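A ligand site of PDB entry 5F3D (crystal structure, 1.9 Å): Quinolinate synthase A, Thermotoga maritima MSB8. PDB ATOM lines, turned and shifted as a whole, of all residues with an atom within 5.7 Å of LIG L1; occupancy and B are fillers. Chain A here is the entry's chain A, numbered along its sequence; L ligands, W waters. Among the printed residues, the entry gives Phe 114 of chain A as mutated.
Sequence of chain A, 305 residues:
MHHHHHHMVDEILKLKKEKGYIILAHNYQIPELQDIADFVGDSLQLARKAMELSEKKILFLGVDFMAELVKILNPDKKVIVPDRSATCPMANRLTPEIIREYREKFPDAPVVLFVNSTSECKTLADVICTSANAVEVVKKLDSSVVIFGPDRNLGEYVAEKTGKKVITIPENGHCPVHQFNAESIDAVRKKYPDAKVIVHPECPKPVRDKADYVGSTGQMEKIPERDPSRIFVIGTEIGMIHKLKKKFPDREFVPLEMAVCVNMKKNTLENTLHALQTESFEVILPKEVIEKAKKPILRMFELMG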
ATOM      1  N   HIS A  26       4.004 -20.315 -23.019  1.00  0.00           N
ATOM      2  CA  HIS A  26       4.060 -19.478 -24.177  1.00  0.00           C
ATOM      3  C   HIS A  26       4.753 -20.230 -25.341  1.00  0.00           C
ATOM      4  O   HIS A  26       5.595 -21.157 -25.121  1.00  0.00           O
ATOM      5  CB  HIS A  26       4.772 -18.186 -23.866  1.00  0.00           C
ATOM      6  CG  HIS A  26       4.697 -17.186 -24.977  1.00  0.00           C
ATOM      7  ND1 HIS A  26       5.616 -17.148 -26.011  1.00  0.00           N
ATOM      8  CD2 HIS A  26       3.822 -16.176 -25.225  1.00  0.00           C
ATOM      9  CE1 HIS A  26       5.320 -16.163 -26.835  1.00  0.00           C
ATOM     10  NE2 HIS A  26       4.219 -15.578 -26.409  1.00  0.00           N
ATOM     11  N   ASN A  27       4.368 -19.836 -26.561  1.00  0.00           N
ATOM     12  CA  ASN A  27       4.924 -20.422 -27.794  1.00  0.00           C
ATOM     13  C   ASN A  27       6.464 -20.382 -27.914  1.00  0.00           C
ATOM     14  O   ASN A  27       7.025 -21.105 -28.719  1.00  0.00           O
ATOM     15  CB  ASN A  27       4.341 -19.721 -29.006  1.00  0.00           C
ATOM     16  CG  ASN A  27       2.864 -20.035 -29.208  1.00  0.00           C
ATOM     17  OD1 ASN A  27       2.388 -21.133 -28.940  1.00  0.00           O
ATOM     18  ND2 ASN A  27       2.144 -19.049 -29.702  1.00  0.00           N
ATOM     19  N   TYR A  28       7.146 -19.565 -27.120  1.00  0.00           N
ATOM     20  CA  TYR A  28       8.589 -19.417 -27.246  1.00  0.00           C
ATOM     21  C   TYR A  28       9.342 -20.259 -26.194  1.00  0.00           C
ATOM     22  O   TYR A  28      10.554 -20.199 -26.100  1.00  0.00           O
ATOM     23  CB  TYR A  28       8.988 -17.931 -27.152  1.00  0.00           C
ATOM     24  CG  TYR A  28       8.509 -16.989 -28.233  1.00  0.00           C
ATOM     25  CD1 TYR A  28       7.956 -17.427 -29.419  1.00  0.00           C
ATOM     26  CD2 TYR A  28       8.629 -15.616 -28.071  1.00  0.00           C
ATOM     27  CE1 TYR A  28       7.535 -16.541 -30.388  1.00  0.00           C
ATOM     28  CE2 TYR A  28       8.180 -14.717 -29.007  1.00  0.00           C
ATOM     29  CZ  TYR A  28       7.630 -15.189 -30.161  1.00  0.00           C
ATOM     30  OH  TYR A  28       7.220 -14.291 -31.085  1.00  0.00           O
ATOM     31  N   ASP A  42      -0.067 -17.981 -27.379  1.00  0.00           N
ATOM     32  CA  ASP A  42       0.440 -16.618 -27.255  1.00  0.00           C
ATOM     33  C   ASP A  42      -0.102 -15.965 -26.005  1.00  0.00           C
ATOM     34  O   ASP A  42      -0.871 -16.592 -25.262  1.00  0.00           O
ATOM     35  CB  ASP A  42       0.174 -15.824 -28.534  1.00  0.00           C
ATOM     36  CG  ASP A  42      -1.337 -15.503 -28.785  1.00  0.00           C
ATOM     37  OD1 ASP A  42      -2.190 -15.790 -27.914  1.00  0.00           O
ATOM     38  OD2 ASP A  42      -1.638 -14.946 -29.882  1.00  0.00           O
ATOM     39  N   SER A  43       0.321 -14.741 -25.732  1.00  0.00           N
ATOM     40  CA  SER A  43      -0.112 -14.036 -24.542  1.00  0.00           C
ATOM     41  C   SER A  43      -1.621 -13.916 -24.451  1.00  0.00           C
ATOM     42  O   SER A  43      -2.169 -14.083 -23.368  1.00  0.00           O
ATOM     43  CB  SER A  43       0.487 -12.608 -24.483  1.00  0.00           C
ATOM     44  OG  SER A  43       1.843 -12.720 -24.170  1.00  0.00           O
ATOM     45  N   LEU A  44      -2.285 -13.648 -25.583  1.00  0.00           N
ATOM     46  CA  LEU A  44      -3.747 -13.413 -25.611  1.00  0.00           C
ATOM     47  C   LEU A  44      -4.488 -14.703 -25.251  1.00  0.00           C
ATOM     48  O   LEU A  44      -5.365 -14.716 -24.371  1.00  0.00           O
ATOM     49  CB  LEU A  44      -4.191 -12.915 -27.004  1.00  0.00           C
ATOM     50  CG  LEU A  44      -5.670 -12.564 -27.224  1.00  0.00           C
ATOM     51  CD1 LEU A  44      -6.148 -11.509 -26.207  1.00  0.00           C
ATOM     52  CD2 LEU A  44      -5.949 -12.102 -28.661  1.00  0.00           C
ATOM     53  N   MET A  66       3.827 -11.472 -18.493  1.00  0.00           N
ATOM     54  CA  MET A  66       2.758 -12.378 -18.875  1.00  0.00           C
ATOM     55  C   MET A  66       2.210 -13.115 -17.679  1.00  0.00           C
ATOM     56  O   MET A  66       0.977 -13.253 -17.561  1.00  0.00           O
ATOM     57  CB  MET A  66       3.230 -13.407 -19.924  1.00  0.00           C
ATOM     58  CG  MET A  66       3.665 -12.802 -21.263  1.00  0.00           C
ATOM     59  SD  MET A  66       4.434 -14.066 -22.362  1.00  0.00           S
ATOM     60  CE  MET A  66       4.929 -12.983 -23.672  1.00  0.00           C
ATOM     61  N   MET A  90      12.642  -5.123 -23.207  1.00  0.00           N
ATOM     62  CA  MET A  90      12.030  -3.990 -23.885  1.00  0.00           C
ATOM     63  C   MET A  90      11.154  -3.151 -22.933  1.00  0.00           C
ATOM     64  O   MET A  90      11.171  -1.927 -22.995  1.00  0.00           O
ATOM     65  CB  MET A  90      11.174  -4.510 -25.040  1.00  0.00           C
ATOM     66  CG  MET A  90      10.591  -3.445 -25.951  1.00  0.00           C
ATOM     67  SD  MET A  90       9.823  -4.196 -27.399  1.00  0.00           S
ATOM     68  CE  MET A  90       8.463  -5.130 -26.667  1.00  0.00           C
ATOM     69  N   PHE A 114       1.372  -2.435 -24.656  1.00  0.00           N
ATOM     70  CA  PHE A 114       1.594  -3.801 -25.119  1.00  0.00           C
ATOM     71  C   PHE A 114       1.776  -4.654 -23.867  1.00  0.00           C
ATOM     72  O   PHE A 114       2.183  -4.169 -22.799  1.00  0.00           O
ATOM     73  CB  PHE A 114       2.824  -3.746 -26.057  1.00  0.00           C
ATOM     74  CG  PHE A 114       3.244  -5.056 -26.657  1.00  0.00           C
ATOM     75  CD1 PHE A 114       2.418  -5.736 -27.524  1.00  0.00           C
ATOM     76  CD2 PHE A 114       4.545  -5.548 -26.443  1.00  0.00           C
ATOM     77  CE1 PHE A 114       2.849  -6.924 -28.119  1.00  0.00           C
ATOM     78  CE2 PHE A 114       4.985  -6.729 -27.024  1.00  0.00           C
ATOM     79  CZ  PHE A 114       4.127  -7.424 -27.871  1.00  0.00           C
ATOM     80  N   VAL A 115       1.410  -5.919 -23.977  1.00  0.00           N
ATOM     81  CA  VAL A 115       1.468  -6.834 -22.838  1.00  0.00           C
ATOM     82  C   VAL A 115       2.840  -6.876 -22.121  1.00  0.00           C
ATOM     83  O   VAL A 115       2.909  -7.138 -20.912  1.00  0.00           O
ATOM     84  CB  VAL A 115       1.074  -8.252 -23.315  1.00  0.00           C
ATOM     85  CG1 VAL A 115       2.106  -8.837 -24.297  1.00  0.00           C
ATOM     86  CG2 VAL A 115       0.843  -9.169 -22.151  1.00  0.00           C
ATOM     87  N   ASN A 116       3.935  -6.663 -22.856  1.00  0.00           N
ATOM     88  CA  ASN A 116       5.254  -6.648 -22.270  1.00  0.00           C
ATOM     89  C   ASN A 116       5.550  -5.255 -21.813  1.00  0.00           C
ATOM     90  O   ASN A 116       6.281  -4.495 -22.449  1.00  0.00           O
ATOM     91  CB  ASN A 116       6.332  -7.151 -23.256  1.00  0.00           C
ATOM     92  CG  ASN A 116       6.364  -8.673 -23.343  1.00  0.00           C
ATOM     93  OD1 ASN A 116       5.863  -9.382 -22.456  1.00  0.00           O
ATOM     94  ND2 ASN A 116       6.986  -9.198 -24.418  1.00  0.00           N
ATOM     95  N   CYS A 129      -2.851  -4.271 -25.133  1.00  0.00           N
ATOM     96  CA  CYS A 129      -2.980  -5.115 -26.312  1.00  0.00           C
ATOM     97  C   CYS A 129      -1.821  -6.113 -26.383  1.00  0.00           C
ATOM     98  O   CYS A 129      -0.791  -5.987 -25.664  1.00  0.00           O
ATOM     99  CB  CYS A 129      -3.097  -4.267 -27.565  1.00  0.00           C
ATOM    100  SG  CYS A 129      -1.518  -3.520 -28.013  1.00  0.00           S
ATOM    101  N   THR A 130      -2.025  -7.119 -27.212  1.00  0.00           N
ATOM    102  CA  THR A 130      -0.984  -8.089 -27.581  1.00  0.00           C
ATOM    103  C   THR A 130      -0.731  -7.920 -29.080  1.00  0.00           C
ATOM    104  O   THR A 130      -1.470  -7.233 -29.754  1.00  0.00           O
ATOM    105  CB  THR A 130      -1.434  -9.547 -27.302  1.00  0.00           C
ATOM    106  OG1 THR A 130      -2.446  -9.925 -28.241  1.00  0.00           O
ATOM    107  CG2 THR A 130      -1.967  -9.692 -25.858  1.00  0.00           C
ATOM    108  N   SER A 131       0.288  -8.599 -29.607  1.00  0.00           N
ATOM    109  CA  SER A 131       0.624  -8.498 -31.051  1.00  0.00           C
ATOM    110  C   SER A 131      -0.553  -8.928 -31.885  1.00  0.00           C
ATOM    111  O   SER A 131      -0.757  -8.428 -32.963  1.00  0.00           O
ATOM    112  CB  SER A 131       1.825  -9.376 -31.400  1.00  0.00           C
ATOM    113  OG  SER A 131       2.799  -9.349 -30.376  1.00  0.00           O
ATOM    114  N   ALA A 132      -1.318  -9.878 -31.347  1.00  0.00           N
ATOM    115  CA  ALA A 132      -2.406 -10.477 -32.063  1.00  0.00           C
ATOM    116  C   ALA A 132      -3.596  -9.537 -32.263  1.00  0.00           C
ATOM    117  O   ALA A 132      -4.279  -9.660 -33.263  1.00  0.00           O
ATOM    118  CB  ALA A 132      -2.841 -11.754 -31.346  1.00  0.00           C
ATOM    119  N   CYS A 175      12.245  -5.219 -29.980  1.00  0.00           N
ATOM    120  CA  CYS A 175      12.570  -6.604 -29.586  1.00  0.00           C
ATOM    121  C   CYS A 175      13.782  -7.118 -30.384  1.00  0.00           C
ATOM    122  O   CYS A 175      13.657  -7.297 -31.600  1.00  0.00           O
ATOM    123  CB  CYS A 175      11.384  -7.511 -29.868  1.00  0.00           C
ATOM    124  SG  CYS A 175      11.803  -9.262 -29.766  1.00  0.00           S
ATOM    125  N   HIS A 178      13.545 -10.019 -33.003  1.00  0.00           N
ATOM    126  CA  HIS A 178      12.826  -9.887 -34.290  1.00  0.00           C
ATOM    127  C   HIS A 178      13.517  -8.966 -35.291  1.00  0.00           C
ATOM    128  O   HIS A 178      12.931  -8.573 -36.312  1.00  0.00           O
ATOM    129  CB  HIS A 178      11.373  -9.434 -34.039  1.00  0.00           C
ATOM    130  CG  HIS A 178      10.498 -10.511 -33.506  1.00  0.00           C
ATOM    131  ND1 HIS A 178      10.240 -10.673 -32.165  1.00  0.00           N
ATOM    132  CD2 HIS A 178       9.870 -11.534 -34.131  1.00  0.00           C
ATOM    133  CE1 HIS A 178       9.471 -11.729 -31.997  1.00  0.00           C
ATOM    134  NE2 HIS A 178       9.223 -12.265 -33.174  1.00  0.00           N
ATOM    135  N   HIS A 200       6.666 -11.570 -37.981  1.00  0.00           N
ATOM    136  CA  HIS A 200       6.035 -10.948 -36.822  1.00  0.00           C
ATOM    137  C   HIS A 200       5.938  -9.470 -37.061  1.00  0.00           C
ATOM    138  O   HIS A 200       6.840  -8.921 -37.670  1.00  0.00           O
ATOM    139  CB  HIS A 200       6.907 -11.197 -35.574  1.00  0.00           C
ATOM    140  CG  HIS A 200       6.140 -11.131 -34.302  1.00  0.00           C
ATOM    141  ND1 HIS A 200       5.934  -9.958 -33.607  1.00  0.00           N
ATOM    142  CD2 HIS A 200       5.506 -12.098 -33.608  1.00  0.00           C
ATOM    143  CE1 HIS A 200       5.212 -10.205 -32.527  1.00  0.00           C
ATOM    144  NE2 HIS A 200       4.958 -11.502 -32.498  1.00  0.00           N
ATOM    145  N   GLU A 202       6.614  -7.215 -34.991  1.00  0.00           N
ATOM    146  CA  GLU A 202       7.781  -6.633 -34.303  1.00  0.00           C
ATOM    147  C   GLU A 202       9.032  -6.568 -35.192  1.00  0.00           C
ATOM    148  O   GLU A 202      10.008  -5.874 -34.843  1.00  0.00           O
ATOM    149  CB  GLU A 202       8.105  -7.402 -33.015  1.00  0.00           C
ATOM    150  CG  GLU A 202       7.131  -7.124 -31.897  1.00  0.00           C
ATOM    151  CD  GLU A 202       7.278  -8.065 -30.721  1.00  0.00           C
ATOM    152  OE1 GLU A 202       8.367  -8.697 -30.544  1.00  0.00           O
ATOM    153  OE2 GLU A 202       6.279  -8.209 -29.986  1.00  0.00           O
ATOM    154  N   SER A 216       1.163 -12.148 -35.602  1.00  0.00           N
ATOM    155  CA  SER A 216       1.578 -12.619 -34.301  1.00  0.00           C
ATOM    156  C   SER A 216       1.679 -14.140 -34.366  1.00  0.00           C
ATOM    157  O   SER A 216       1.196 -14.719 -35.345  1.00  0.00           O
ATOM    158  CB  SER A 216       0.512 -12.213 -33.302  1.00  0.00           C
ATOM    159  OG  SER A 216      -0.654 -12.990 -33.492  1.00  0.00           O
ATOM    160  N   THR A 217       2.233 -14.786 -33.329  1.00  0.00           N
ATOM    161  CA  THR A 217       2.353 -16.255 -33.335  1.00  0.00           C
ATOM    162  C   THR A 217       0.980 -16.927 -33.429  1.00  0.00           C
ATOM    163  O   THR A 217       0.821 -17.955 -34.139  1.00  0.00           O
ATOM    164  CB  THR A 217       3.148 -16.841 -32.149  1.00  0.00           C
ATOM    165  OG1 THR A 217       2.493 -16.543 -30.890  1.00  0.00           O
ATOM    166  CG2 THR A 217       4.576 -16.298 -32.146  1.00  0.00           C
ATOM    167  N   GLY A 218       0.009 -16.404 -32.702  1.00  0.00           N
ATOM    168  CA  GLY A 218      -1.382 -16.874 -32.797  1.00  0.00           C
ATOM    169  C   GLY A 218      -1.940 -16.861 -34.226  1.00  0.00           C
ATOM    170  O   GLY A 218      -2.585 -17.794 -34.676  1.00  0.00           O
ATOM    171  N   THR A 236      10.021 -15.447 -36.610  1.00  0.00           N
ATOM    172  CA  THR A 236       9.832 -15.158 -35.185  1.00  0.00           C
ATOM    173  C   THR A 236      10.825 -15.991 -34.415  1.00  0.00           C
ATOM    174  O   THR A 236      11.713 -16.609 -35.023  1.00  0.00           O
ATOM    175  CB  THR A 236       8.348 -15.348 -34.748  1.00  0.00           C
ATOM    176  OG1 THR A 236       8.128 -14.671 -33.503  1.00  0.00           O
ATOM    177  CG2 THR A 236       7.971 -16.833 -34.594  1.00  0.00           C
ATOM    178  N   MET A 264      12.974 -16.181 -22.405  1.00  0.00           N
ATOM    179  CA  MET A 264      12.076 -17.283 -22.603  1.00  0.00           C
ATOM    180  C   MET A 264      12.753 -18.625 -22.370  1.00  0.00           C
ATOM    181  O   MET A 264      12.151 -19.561 -21.855  1.00  0.00           O
ATOM    182  CB  MET A 264      11.503 -17.236 -24.025  1.00  0.00           C
ATOM    183  CG  MET A 264      10.458 -16.157 -24.219  1.00  0.00           C
ATOM    184  SD  MET A 264       8.924 -16.623 -23.374  1.00  0.00           S
ATOM    185  CE  MET A 264       7.773 -15.380 -23.923  1.00  0.00           C
HETATM  186  O1  LIG L   1       1.274 -10.528 -27.795  1.00  0.00           O
HETATM  187  C1  LIG L   1       1.678 -11.522 -28.404  1.00  0.00           C
HETATM  188  O2  LIG L   1       1.122 -11.912 -29.432  1.00  0.00           O
HETATM  189  C2  LIG L   1       2.821 -12.221 -27.898  1.00  0.00           C
HETATM  190  N1  LIG L   1       2.647 -12.564 -26.714  1.00  0.00           N
HETATM  191  C3  LIG L   1       4.032 -12.672 -28.706  1.00  0.00           C
HETATM  192  C4  LIG L   1       3.405 -13.364 -29.847  1.00  0.00           C
HETATM  193  O3  LIG L   1       3.530 -13.059 -31.048  1.00  0.00           O
HETATM  194  O4  LIG L   1       2.718 -14.283 -29.504  1.00  0.00           O
HETATM  195  C5  LIG L   1       5.107 -11.691 -29.200  1.00  0.00           C
HETATM  196  C6  LIG L   1       5.941 -11.032 -28.132  1.00  0.00           C
HETATM  197  C7  LIG L   1       6.046 -11.470 -26.706  1.00  0.00           C
HETATM  198  O5  LIG L   1       7.215 -12.259 -26.508  1.00  0.00           O
HETATM  199  O6  LIG L   1       6.573 -10.054 -28.417  1.00  0.00           O
HETATM  200 FE1  LG2 L   2      11.218 -10.160 -27.705  1.00  0.00          FE
HETATM  201 FE2  LG2 L   2      11.769 -11.920 -25.658  1.00  0.00          FE
HETATM  202 FE3  LG2 L   2       9.065 -11.366 -26.503  1.00  0.00          FE
HETATM  203 FE4  LG2 L   2      10.488  -9.547 -25.049  1.00  0.00          FE
HETATM  204  S1  LG2 L   2       9.840 -11.532 -24.288  1.00  0.00           S
HETATM  205  S2  LG2 L   2       9.252  -9.147 -27.098  1.00  0.00           S
HETATM  206  S3  LG2 L   2      12.700  -9.884 -25.880  1.00  0.00           S
HETATM  207  S4  LG2 L   2      10.848 -12.401 -27.775  1.00  0.00           S
HETATM  208  O   HOH W   1       0.369 -13.949 -31.008  1.00  0.00           O
HETATM  209  O   HOH W   2      -1.232 -12.535 -28.489  1.00  0.00           O
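The side-chain amide nitrogen of Asn 27 is in hydrogen-bond range of the side-chain hydroxyl of Thr 217, at 2.8 Å. OG1 of Thr 130 lies close to N of Ala 132 (3.3 Å). The side-chain sulfur (SD) of Met 66 sits close to the side-chain hydroxyl (OG) of Ser 43 (3.4 Å). A ring nitrogen (ND1) of His 26 lies close to the backbone NH of Tyr 28, 3.1 Å away. The side-chain carboxylate of Asp 42 sits at hydrogen-bond distance from the backbone NH of Leu 44, 3.2 Å away. SG of Cys 175 sits close to OE1 of Glu 202, 3.6 Å away. N of Asp 42 lies close to ND2 of Asn 27, at 3.4 Å. A ring nitrogen (ND1) of His 178 is in hydrogen-bond range of the side-chain carboxylate (OE1) of Glu 202, 3.2 Å away.
Water W2 lies within hydrogen-bond range of O2 of LIG L1 (2.6 Å), OD2 of Asp 42 (2.8 Å), OG1 of Thr 130 (2.9 Å) and N of Leu 44 (3.3 Å). Water W1 lies within hydrogen-bond range of OD2 of Asp 42 (2.5 Å), O2 of LIG L1 (2.7 Å), OG of Ser 216 (2.9 Å), N of Gly 218 (3.0 Å) and N of Thr 217 (3.1 Å).
ND2 of Asn 116 lies close to S2 of LG2 L2 (3.5 Å). An oxygen (O2) of LIG L1 lies close to the side-chain hydroxyl of Ser 131. The side-chain carboxylate of Glu 202 sits close to an oxygen (O6) of LIG L1, at 2.4 Å. The side-chain sulfur (SG) of Cys 175 is bound to an iron atom (FE1) of LG2 L2, 2.3 Å away. An oxygen (O3) of LIG L1 lies within hydrogen-bond range of a ring nitrogen (NE2) of His 200 (2.6 Å). The backbone NH of Ser 43 lies close to a nitrogen (N1) of LIG L1, 3.3 Å away. An oxygen (O4) of LIG L1 sits at hydrogen-bond distance from the side-chain hydroxyl of Thr 217, at 2.7 Å. The backbone NH of Ser 131 sits at hydrogen-bond distance from an oxygen (O1) of LIG L1, at 2.8 Å. N1 of LIG L1 lies within hydrogen-bond range of NE2 of His 26, 3.4 Å away. The backbone NH (N) of Thr 217 is in hydrogen-bond range of an oxygen (O3) of LIG L1 (3.1 Å). The side-chain hydroxyl (OG) of Ser 43 is in hydrogen-bond range of a nitrogen (N1) of LIG L1, at 2.7 Å.
Merely in contact with LIG L1: Tyr 28, Asp 42, Met 66, Phe 114, Val 115, Asn 116, Thr 130, Ala 132 and Ser 216. Hydrophobic or aromatic side chains within 4 Å of LIG L1: Tyr 28, Met 66, Phe 114, Val 115 and His 200. The nearest printed residue that does not touch LIG L1 is Met 264 (4.1 Å).
An oxygen (O5) of LIG L1 binds an iron atom (FE3) of LG2 L2, 2.1 Å away.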
